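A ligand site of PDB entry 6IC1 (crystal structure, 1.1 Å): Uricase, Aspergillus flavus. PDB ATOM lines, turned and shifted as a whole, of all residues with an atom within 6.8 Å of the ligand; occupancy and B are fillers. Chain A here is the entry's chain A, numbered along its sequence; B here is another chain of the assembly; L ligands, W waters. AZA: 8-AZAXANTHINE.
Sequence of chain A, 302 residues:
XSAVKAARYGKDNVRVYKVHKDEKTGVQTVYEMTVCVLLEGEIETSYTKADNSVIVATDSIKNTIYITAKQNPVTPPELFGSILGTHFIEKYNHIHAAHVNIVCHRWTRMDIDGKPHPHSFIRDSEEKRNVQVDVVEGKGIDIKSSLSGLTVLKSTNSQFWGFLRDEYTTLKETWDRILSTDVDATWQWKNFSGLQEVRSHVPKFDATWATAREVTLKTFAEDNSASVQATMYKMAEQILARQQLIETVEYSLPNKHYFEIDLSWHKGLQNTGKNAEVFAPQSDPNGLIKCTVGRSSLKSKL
The backbone NH (N) of Thr 58 of chain B is in hydrogen-bond range of a nitrogen (N7) of the ligand, at 2.8 Å. N8 of the ligand is in hydrogen-bond range of OG1 of Thr 58 of chain B (3.2 Å). An oxygen (O2) of the ligand sits at hydrogen-bond distance from the guanidinium group (NH2) of Arg 177 (2.8 Å). O6 of the ligand sits at hydrogen-bond distance from NE2 of Gln 229. N of Val 228 is in hydrogen-bond range of O2 of the ligand, at 2.9 Å. ND2 of Asn 255 lies close to N3 of the ligand (3.2 Å).
The side-chain hydroxyl (OG1) of Thr 58 of chain B sits at hydrogen-bond distance from the side-chain amino group (NZ) of Lys 11 of chain B (2.7 Å). N of Arg 177 lies within hydrogen-bond range of O of Ser 158 (2.9 Å). OG of Ser 227 lies close to N of Gln 229. A ring nitrogen (NE2) of His 257 sits at hydrogen-bond distance from the backbone carbonyl oxygen (O) of Asn 255. O of Gly 287 lies within hydrogen-bond range of N of Asn 255. The backbone carbonyl oxygen (O) of Ser 227 lies within hydrogen-bond range of the side-chain hydroxyl (OG) of Ser 225, 2.9 Å away. The backbone carbonyl oxygen (O) of Val 56 of chain B is in hydrogen-bond range of the side-chain hydroxyl (OH) of Tyr 9 of chain B, 2.6 Å away.
Residues that only touch the ligand: Phe 160, Ile 55 of chain B, Ser 227, Ala 57 of chain B, Leu 171, Tyr 9 of chain B and Asp 59 of chain B. Of the 26 residues printed, 12 come within 4 Å of the ligand.
Water W2 bridges a nitrogen (N9) of the ligand and the guanidinium group (NH1) of Arg 177. Water W1 bridges the side-chain hydroxyl of Thr 58 of chain B and the side-chain amide nitrogen of Asn 255.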
ATOM      1  N   SER A 158      -9.954 -34.033  -5.159  1.00  0.00           N
ATOM      2  CA  SER A 158     -10.723 -33.444  -6.239  1.00  0.00           C
ATOM      3  C   SER A 158     -10.876 -34.520  -7.280  1.00  0.00           C
ATOM      4  O   SER A 158      -9.931 -35.257  -7.569  1.00  0.00           O
ATOM      5  CB  SER A 158     -10.032 -32.225  -6.794  1.00  0.00           C
ATOM      6  OG  SER A 158     -10.665 -31.737  -7.961  1.00  0.00           O
ATOM      7  N   GLN A 159     -12.086 -34.612  -7.819  1.00  0.00           N
ATOM      8  CA  GLN A 159     -12.486 -35.610  -8.815  1.00  0.00           C
ATOM      9  C   GLN A 159     -13.230 -34.904  -9.959  1.00  0.00           C
ATOM     10  O   GLN A 159     -13.822 -33.842  -9.779  1.00  0.00           O
ATOM     11  CB  GLN A 159     -13.362 -36.686  -8.171  1.00  0.00           C
ATOM     12  CG  GLN A 159     -12.792 -37.203  -6.856  1.00  0.00           C
ATOM     13  CD  GLN A 159     -13.580 -38.347  -6.298  1.00  0.00           C
ATOM     14  OE1 GLN A 159     -14.087 -39.205  -7.023  1.00  0.00           O
ATOM     15  NE2 GLN A 159     -13.614 -38.426  -4.987  1.00  0.00           N
ATOM     16  N   PHE A 160     -13.287 -35.585 -11.100  1.00  0.00           N
ATOM     17  CA  PHE A 160     -14.192 -35.131 -12.147  1.00  0.00           C
ATOM     18  C   PHE A 160     -14.479 -36.299 -13.096  1.00  0.00           C
ATOM     19  O   PHE A 160     -13.664 -36.643 -13.958  1.00  0.00           O
ATOM     20  CB  PHE A 160     -13.650 -33.914 -12.886  1.00  0.00           C
ATOM     21  CG  PHE A 160     -14.679 -33.273 -13.762  1.00  0.00           C
ATOM     22  CD1 PHE A 160     -15.844 -32.734 -13.198  1.00  0.00           C
ATOM     23  CD2 PHE A 160     -14.536 -33.221 -15.122  1.00  0.00           C
ATOM     24  CE1 PHE A 160     -16.777 -32.174 -14.037  1.00  0.00           C
ATOM     25  CE2 PHE A 160     -15.488 -32.627 -15.938  1.00  0.00           C
ATOM     26  CZ  PHE A 160     -16.613 -32.105 -15.391  1.00  0.00           C
ATOM     27  N   PHE A 163     -19.195 -36.834 -16.540  1.00  0.00           N
ATOM     28  CA  PHE A 163     -19.588 -35.770 -17.441  1.00  0.00           C
ATOM     29  C   PHE A 163     -19.977 -36.316 -18.806  1.00  0.00           C
ATOM     30  O   PHE A 163     -19.718 -37.485 -19.159  1.00  0.00           O
ATOM     31  CB  PHE A 163     -18.487 -34.727 -17.518  1.00  0.00           C
ATOM     32  CG  PHE A 163     -17.143 -35.274 -17.900  1.00  0.00           C
ATOM     33  CD1 PHE A 163     -16.758 -35.426 -19.222  1.00  0.00           C
ATOM     34  CD2 PHE A 163     -16.264 -35.637 -16.895  1.00  0.00           C
ATOM     35  CE1 PHE A 163     -15.505 -35.950 -19.512  1.00  0.00           C
ATOM     36  CE2 PHE A 163     -15.011 -36.170 -17.188  1.00  0.00           C
ATOM     37  CZ  PHE A 163     -14.646 -36.328 -18.492  1.00  0.00           C
ATOM     38  N   LEU A 171     -11.457 -35.732 -22.823  1.00  0.00           N
ATOM     39  CA  LEU A 171     -11.026 -35.698 -21.430  1.00  0.00           C
ATOM     40  C   LEU A 171     -11.252 -37.034 -20.748  1.00  0.00           C
ATOM     41  O   LEU A 171     -12.392 -37.539 -20.742  1.00  0.00           O
ATOM     42  CB  LEU A 171     -11.822 -34.614 -20.704  1.00  0.00           C
ATOM     43  CG  LEU A 171     -11.454 -34.381 -19.240  1.00  0.00           C
ATOM     44  CD1 LEU A 171     -10.016 -33.894 -19.075  1.00  0.00           C
ATOM     45  CD2 LEU A 171     -12.404 -33.406 -18.578  1.00  0.00           C
ATOM     46  N   ARG A 177      -7.345 -35.680  -8.793  1.00  0.00           N
ATOM     47  CA  ARG A 177      -6.678 -34.625  -9.567  1.00  0.00           C
ATOM     48  C   ARG A 177      -6.342 -33.475  -8.633  1.00  0.00           C
ATOM     49  O   ARG A 177      -6.809 -33.404  -7.490  1.00  0.00           O
ATOM     50  CB  ARG A 177      -7.511 -34.133 -10.726  1.00  0.00           C
ATOM     51  CG  ARG A 177      -8.807 -33.399 -10.308  1.00  0.00           C
ATOM     52  CD  ARG A 177      -9.586 -32.786 -11.454  1.00  0.00           C
ATOM     53  NE  ARG A 177     -10.724 -32.074 -10.902  1.00  0.00           N
ATOM     54  CZ  ARG A 177     -11.530 -31.316 -11.624  1.00  0.00           C
ATOM     55  NH1 ARG A 177     -11.479 -31.304 -12.927  1.00  0.00           N
ATOM     56  NH2 ARG A 177     -12.427 -30.542 -11.002  1.00  0.00           N
ATOM     57  N   LEU A 179      -6.759 -29.498  -7.821  1.00  0.00           N
ATOM     58  CA  LEU A 179      -7.697 -28.412  -8.055  1.00  0.00           C
ATOM     59  C   LEU A 179      -7.071 -27.113  -7.529  1.00  0.00           C
ATOM     60  O   LEU A 179      -6.688 -27.056  -6.341  1.00  0.00           O
ATOM     61  CB  LEU A 179      -9.014 -28.697  -7.347  1.00  0.00           C
ATOM     62  CG  LEU A 179     -10.072 -27.588  -7.426  1.00  0.00           C
ATOM     63  CD1 LEU A 179     -10.419 -27.272  -8.883  1.00  0.00           C
ATOM     64  CD2 LEU A 179     -11.274 -27.969  -6.611  1.00  0.00           C
ATOM     65  N   SER A 225     -14.092 -33.057  -3.694  1.00  0.00           N
ATOM     66  CA  SER A 225     -14.876 -32.290  -4.678  1.00  0.00           C
ATOM     67  C   SER A 225     -15.278 -33.121  -5.870  1.00  0.00           C
ATOM     68  O   SER A 225     -14.434 -33.718  -6.536  1.00  0.00           O
ATOM     69  CB  SER A 225     -14.037 -31.102  -5.102  1.00  0.00           C
ATOM     70  OG  SER A 225     -14.623 -30.428  -6.201  1.00  0.00           O
ATOM     71  N   ALA A 226     -16.565 -33.093  -6.207  1.00  0.00           N
ATOM     72  CA  ALA A 226     -17.110 -33.738  -7.399  1.00  0.00           C
ATOM     73  C   ALA A 226     -16.879 -32.939  -8.658  1.00  0.00           C
ATOM     74  O   ALA A 226     -16.961 -33.483  -9.760  1.00  0.00           O
ATOM     75  CB  ALA A 226     -18.563 -34.017  -7.223  1.00  0.00           C
ATOM     76  N   SER A 227     -16.681 -31.624  -8.487  1.00  0.00           N
ATOM     77  CA  SER A 227     -16.536 -30.662  -9.571  1.00  0.00           C
ATOM     78  C   SER A 227     -16.349 -29.287  -8.889  1.00  0.00           C
ATOM     79  O   SER A 227     -16.722 -29.113  -7.718  1.00  0.00           O
ATOM     80  CB  SER A 227     -17.736 -30.568 -10.478  1.00  0.00           C
ATOM     81  OG  SER A 227     -18.865 -30.101  -9.749  1.00  0.00           O
ATOM     82  N   VAL A 228     -15.867 -28.336  -9.652  1.00  0.00           N
ATOM     83  CA  VAL A 228     -15.858 -26.952  -9.183  1.00  0.00           C
ATOM     84  C   VAL A 228     -17.276 -26.515  -8.843  1.00  0.00           C
ATOM     85  O   VAL A 228     -17.510 -25.884  -7.801  1.00  0.00           O
ATOM     86  CB  VAL A 228     -15.185 -26.027 -10.185  1.00  0.00           C
ATOM     87  CG1 VAL A 228     -15.243 -24.562  -9.731  1.00  0.00           C
ATOM     88  CG2 VAL A 228     -13.727 -26.415 -10.400  1.00  0.00           C
ATOM     89  N   GLN A 229     -18.201 -26.822  -9.729  1.00  0.00           N
ATOM     90  CA  GLN A 229     -19.611 -26.495  -9.556  1.00  0.00           C
ATOM     91  C   GLN A 229     -20.129 -26.937  -8.196  1.00  0.00           C
ATOM     92  O   GLN A 229     -20.786 -26.158  -7.493  1.00  0.00           O
ATOM     93  CB  GLN A 229     -20.428 -27.164 -10.656  1.00  0.00           C
ATOM     94  CG  GLN A 229     -20.275 -26.604 -12.099  1.00  0.00           C
ATOM     95  CD  GLN A 229     -19.118 -27.145 -12.919  1.00  0.00           C
ATOM     96  OE1 GLN A 229     -18.099 -27.615 -12.396  1.00  0.00           O
ATOM     97  NE2 GLN A 229     -19.275 -27.074 -14.247  1.00  0.00           N
ATOM     98  N   ASN A 255     -10.712 -22.747 -13.326  1.00  0.00           N
ATOM     99  CA  ASN A 255     -10.124 -24.065 -13.034  1.00  0.00           C
ATOM    100  C   ASN A 255      -8.716 -24.019 -13.647  1.00  0.00           C
ATOM    101  O   ASN A 255      -8.587 -24.040 -14.864  1.00  0.00           O
ATOM    102  CB  ASN A 255     -10.981 -25.166 -13.643  1.00  0.00           C
ATOM    103  CG  ASN A 255     -10.627 -26.534 -13.162  1.00  0.00           C
ATOM    104  OD1 ASN A 255      -9.749 -26.691 -12.285  1.00  0.00           O
ATOM    105  ND2 ASN A 255     -11.342 -27.551 -13.662  1.00  0.00           N
ATOM    106  N   HIS A 257      -5.650 -25.422 -14.566  1.00  0.00           N
ATOM    107  CA  HIS A 257      -5.361 -26.839 -14.764  1.00  0.00           C
ATOM    108  C   HIS A 257      -3.874 -27.160 -14.550  1.00  0.00           C
ATOM    109  O   HIS A 257      -2.992 -26.407 -14.950  1.00  0.00           O
ATOM    110  CB  HIS A 257      -5.725 -27.251 -16.207  1.00  0.00           C
ATOM    111  CG  HIS A 257      -7.152 -26.931 -16.570  1.00  0.00           C
ATOM    112  ND1 HIS A 257      -8.250 -27.545 -15.975  1.00  0.00           N
ATOM    113  CD2 HIS A 257      -7.671 -26.019 -17.421  1.00  0.00           C
ATOM    114  CE1 HIS A 257      -9.335 -26.959 -16.489  1.00  0.00           C
ATOM    115  NE2 HIS A 257      -9.032 -26.023 -17.399  1.00  0.00           N
ATOM    116  N   GLY A 287     -10.738 -23.531 -17.503  1.00  0.00           N
ATOM    117  CA  GLY A 287     -12.163 -23.558 -17.203  1.00  0.00           C
ATOM    118  C   GLY A 287     -12.561 -22.280 -16.463  1.00  0.00           C
ATOM    119  O   GLY A 287     -11.745 -21.722 -15.701  1.00  0.00           O
ATOM    120  N   ILE A 289     -15.978 -21.130 -14.196  1.00  0.00           N
ATOM    121  CA  ILE A 289     -17.235 -21.687 -13.627  1.00  0.00           C
ATOM    122  C   ILE A 289     -17.870 -20.570 -12.769  1.00  0.00           C
ATOM    123  O   ILE A 289     -17.196 -20.017 -11.895  1.00  0.00           O
ATOM    124  CB  ILE A 289     -16.938 -22.920 -12.747  1.00  0.00           C
ATOM    125  CG1 ILE A 289     -15.878 -23.865 -13.385  1.00  0.00           C
ATOM    126  CG2 ILE A 289     -18.228 -23.627 -12.435  1.00  0.00           C
ATOM    127  CD1 ILE A 289     -16.211 -24.490 -14.682  1.00  0.00           C
ATOM    128  N   TYR B   9     -20.893 -21.572 -17.409  1.00  0.00           N
ATOM    129  CA  TYR B   9     -19.566 -22.186 -17.251  1.00  0.00           C
ATOM    130  C   TYR B   9     -19.017 -22.501 -18.608  1.00  0.00           C
ATOM    131  O   TYR B   9     -19.758 -22.718 -19.585  1.00  0.00           O
ATOM    132  CB  TYR B   9     -19.641 -23.435 -16.353  1.00  0.00           C
ATOM    133  CG  TYR B   9     -20.061 -24.653 -17.122  1.00  0.00           C
ATOM    134  CD1 TYR B   9     -21.355 -24.833 -17.587  1.00  0.00           C
ATOM    135  CD2 TYR B   9     -19.120 -25.544 -17.573  1.00  0.00           C
ATOM    136  CE1 TYR B   9     -21.695 -25.816 -18.482  1.00  0.00           C
ATOM    137  CE2 TYR B   9     -19.400 -26.526 -18.476  1.00  0.00           C
ATOM    138  CZ  TYR B   9     -20.692 -26.655 -18.966  1.00  0.00           C
ATOM    139  OH  TYR B   9     -21.020 -27.597 -19.888  1.00  0.00           O
ATOM    140  N   GLY B  10     -17.710 -22.630 -18.701  1.00  0.00           N
ATOM    141  CA  GLY B  10     -17.113 -23.003 -19.961  1.00  0.00           C
ATOM    142  C   GLY B  10     -15.616 -22.829 -19.939  1.00  0.00           C
ATOM    143  O   GLY B  10     -14.991 -23.019 -18.888  1.00  0.00           O
ATOM    144  N   LYS B  11     -15.044 -22.523 -21.103  1.00  0.00           N
ATOM    145  CA  LYS B  11     -13.588 -22.404 -21.220  1.00  0.00           C
ATOM    146  C   LYS B  11     -13.261 -20.981 -21.624  1.00  0.00           C
ATOM    147  O   LYS B  11     -13.783 -20.459 -22.606  1.00  0.00           O
ATOM    148  CB  LYS B  11     -12.977 -23.411 -22.230  1.00  0.00           C
ATOM    149  CG  LYS B  11     -11.482 -23.516 -22.055  1.00  0.00           C
ATOM    150  CD  LYS B  11     -11.041 -24.306 -20.885  1.00  0.00           C
ATOM    151  CE  LYS B  11     -10.824 -25.777 -21.135  1.00  0.00           C
ATOM    152  NZ  LYS B  11     -10.864 -26.570 -19.881  1.00  0.00           N
ATOM    153  N   ASN B  52     -22.812 -34.563 -12.798  1.00  0.00           N
ATOM    154  CA  ASN B  52     -21.957 -34.148 -13.906  1.00  0.00           C
ATOM    155  C   ASN B  52     -22.551 -34.531 -15.260  1.00  0.00           C
ATOM    156  O   ASN B  52     -21.996 -34.099 -16.272  1.00  0.00           O
ATOM    157  CB  ASN B  52     -20.524 -34.596 -13.750  1.00  0.00           C
ATOM    158  CG  ASN B  52     -19.837 -33.916 -12.607  1.00  0.00           C
ATOM    159  OD1 ASN B  52     -20.154 -32.734 -12.345  1.00  0.00           O
ATOM    160  ND2 ASN B  52     -18.845 -34.562 -11.978  1.00  0.00           N
ATOM    161  N   ILE B  55     -22.996 -31.742 -17.686  1.00  0.00           N
ATOM    162  CA  ILE B  55     -21.831 -30.923 -18.034  1.00  0.00           C
ATOM    163  C   ILE B  55     -21.199 -31.410 -19.334  1.00  0.00           C
ATOM    164  O   ILE B  55     -20.681 -32.555 -19.397  1.00  0.00           O
ATOM    165  CB  ILE B  55     -20.789 -30.895 -16.917  1.00  0.00           C
ATOM    166  CG1 ILE B  55     -21.348 -30.319 -15.604  1.00  0.00           C
ATOM    167  CG2 ILE B  55     -19.566 -30.154 -17.377  1.00  0.00           C
ATOM    168  CD1 ILE B  55     -20.353 -30.487 -14.473  1.00  0.00           C
ATOM    169  N   VAL B  56     -21.218 -30.544 -20.341  1.00  0.00           N
ATOM    170  CA  VAL B  56     -20.351 -30.610 -21.505  1.00  0.00           C
ATOM    171  C   VAL B  56     -18.995 -30.117 -21.000  1.00  0.00           C
ATOM    172  O   VAL B  56     -18.875 -28.961 -20.589  1.00  0.00           O
ATOM    173  CB  VAL B  56     -20.889 -29.756 -22.665  1.00  0.00           C
ATOM    174  CG1 VAL B  56     -19.911 -29.790 -23.783  1.00  0.00           C
ATOM    175  CG2 VAL B  56     -22.264 -30.222 -23.097  1.00  0.00           C
ATOM    176  N   ALA B  57     -18.008 -30.986 -20.899  1.00  0.00           N
ATOM    177  CA  ALA B  57     -16.778 -30.608 -20.182  1.00  0.00           C
ATOM    178  C   ALA B  57     -16.166 -29.358 -20.812  1.00  0.00           C
ATOM    179  O   ALA B  57     -16.178 -29.161 -22.029  1.00  0.00           O
ATOM    180  CB  ALA B  57     -15.780 -31.743 -20.199  1.00  0.00           C
ATOM    181  N   THR B  58     -15.561 -28.529 -19.957  1.00  0.00           N
ATOM    182  CA  THR B  58     -14.872 -27.363 -20.510  1.00  0.00           C
ATOM    183  C   THR B  58     -13.798 -27.764 -21.503  1.00  0.00           C
ATOM    184  O   THR B  58     -13.586 -27.125 -22.523  1.00  0.00           O
ATOM    185  CB  THR B  58     -14.336 -26.446 -19.390  1.00  0.00           C
ATOM    186  OG1 THR B  58     -13.244 -27.056 -18.694  1.00  0.00           O
ATOM    187  CG2 THR B  58     -15.422 -26.108 -18.398  1.00  0.00           C
ATOM    188  N   ASP B  59     -13.123 -28.901 -21.219  1.00  0.00           N
ATOM    189  CA  ASP B  59     -12.115 -29.428 -22.154  1.00  0.00           C
ATOM    190  C   ASP B  59     -12.755 -29.717 -23.527  1.00  0.00           C
ATOM    191  O   ASP B  59     -12.118 -29.512 -24.566  1.00  0.00           O
ATOM    192  CB  ASP B  59     -11.517 -30.703 -21.570  1.00  0.00           C
ATOM    193  CG  ASP B  59     -10.357 -31.166 -22.372  1.00  0.00           C
ATOM    194  OD1 ASP B  59      -9.227 -30.609 -22.167  1.00  0.00           O
ATOM    195  OD2 ASP B  59     -10.515 -32.082 -23.206  1.00  0.00           O
ATOM    196  N   SER B  60     -13.986 -30.241 -23.520  1.00  0.00           N
ATOM    197  CA  SER B  60     -14.706 -30.507 -24.770  1.00  0.00           C
ATOM    198  C   SER B  60     -15.102 -29.214 -25.481  1.00  0.00           C
ATOM    199  O   SER B  60     -15.121 -29.179 -26.692  1.00  0.00           O
ATOM    200  CB  SER B  60     -15.961 -31.360 -24.499  1.00  0.00           C
ATOM    201  OG  SER B  60     -15.572 -32.557 -23.817  1.00  0.00           O
HETATM  202  N1  AZA L   1     -15.826 -28.719 -14.033  1.00  0.00           N
HETATM  203  C2  AZA L   1     -14.719 -29.211 -13.368  1.00  0.00           C
HETATM  204  O2  AZA L   1     -14.669 -29.213 -12.134  1.00  0.00           O
HETATM  205  N3  AZA L   1     -13.701 -29.714 -14.134  1.00  0.00           N
HETATM  206  C4  AZA L   1     -13.912 -29.742 -15.446  1.00  0.00           C
HETATM  207  C5  AZA L   1     -15.031 -29.297 -16.097  1.00  0.00           C
HETATM  208  C6  AZA L   1     -16.115 -28.708 -15.386  1.00  0.00           C
HETATM  209  O6  AZA L   1     -17.154 -28.218 -15.816  1.00  0.00           O
HETATM  210  N7  AZA L   1     -14.877 -29.496 -17.442  1.00  0.00           N
HETATM  211  N8  AZA L   1     -13.695 -30.035 -17.653  1.00  0.00           N
HETATM  212  N9  AZA L   1     -13.110 -30.186 -16.440  1.00  0.00           N
HETATM  213  O   HOH W   1     -13.030 -26.631 -15.951  1.00  0.00           O
HETATM  214  O   HOH W   2     -10.430 -30.958 -16.097  1.00  0.00           O
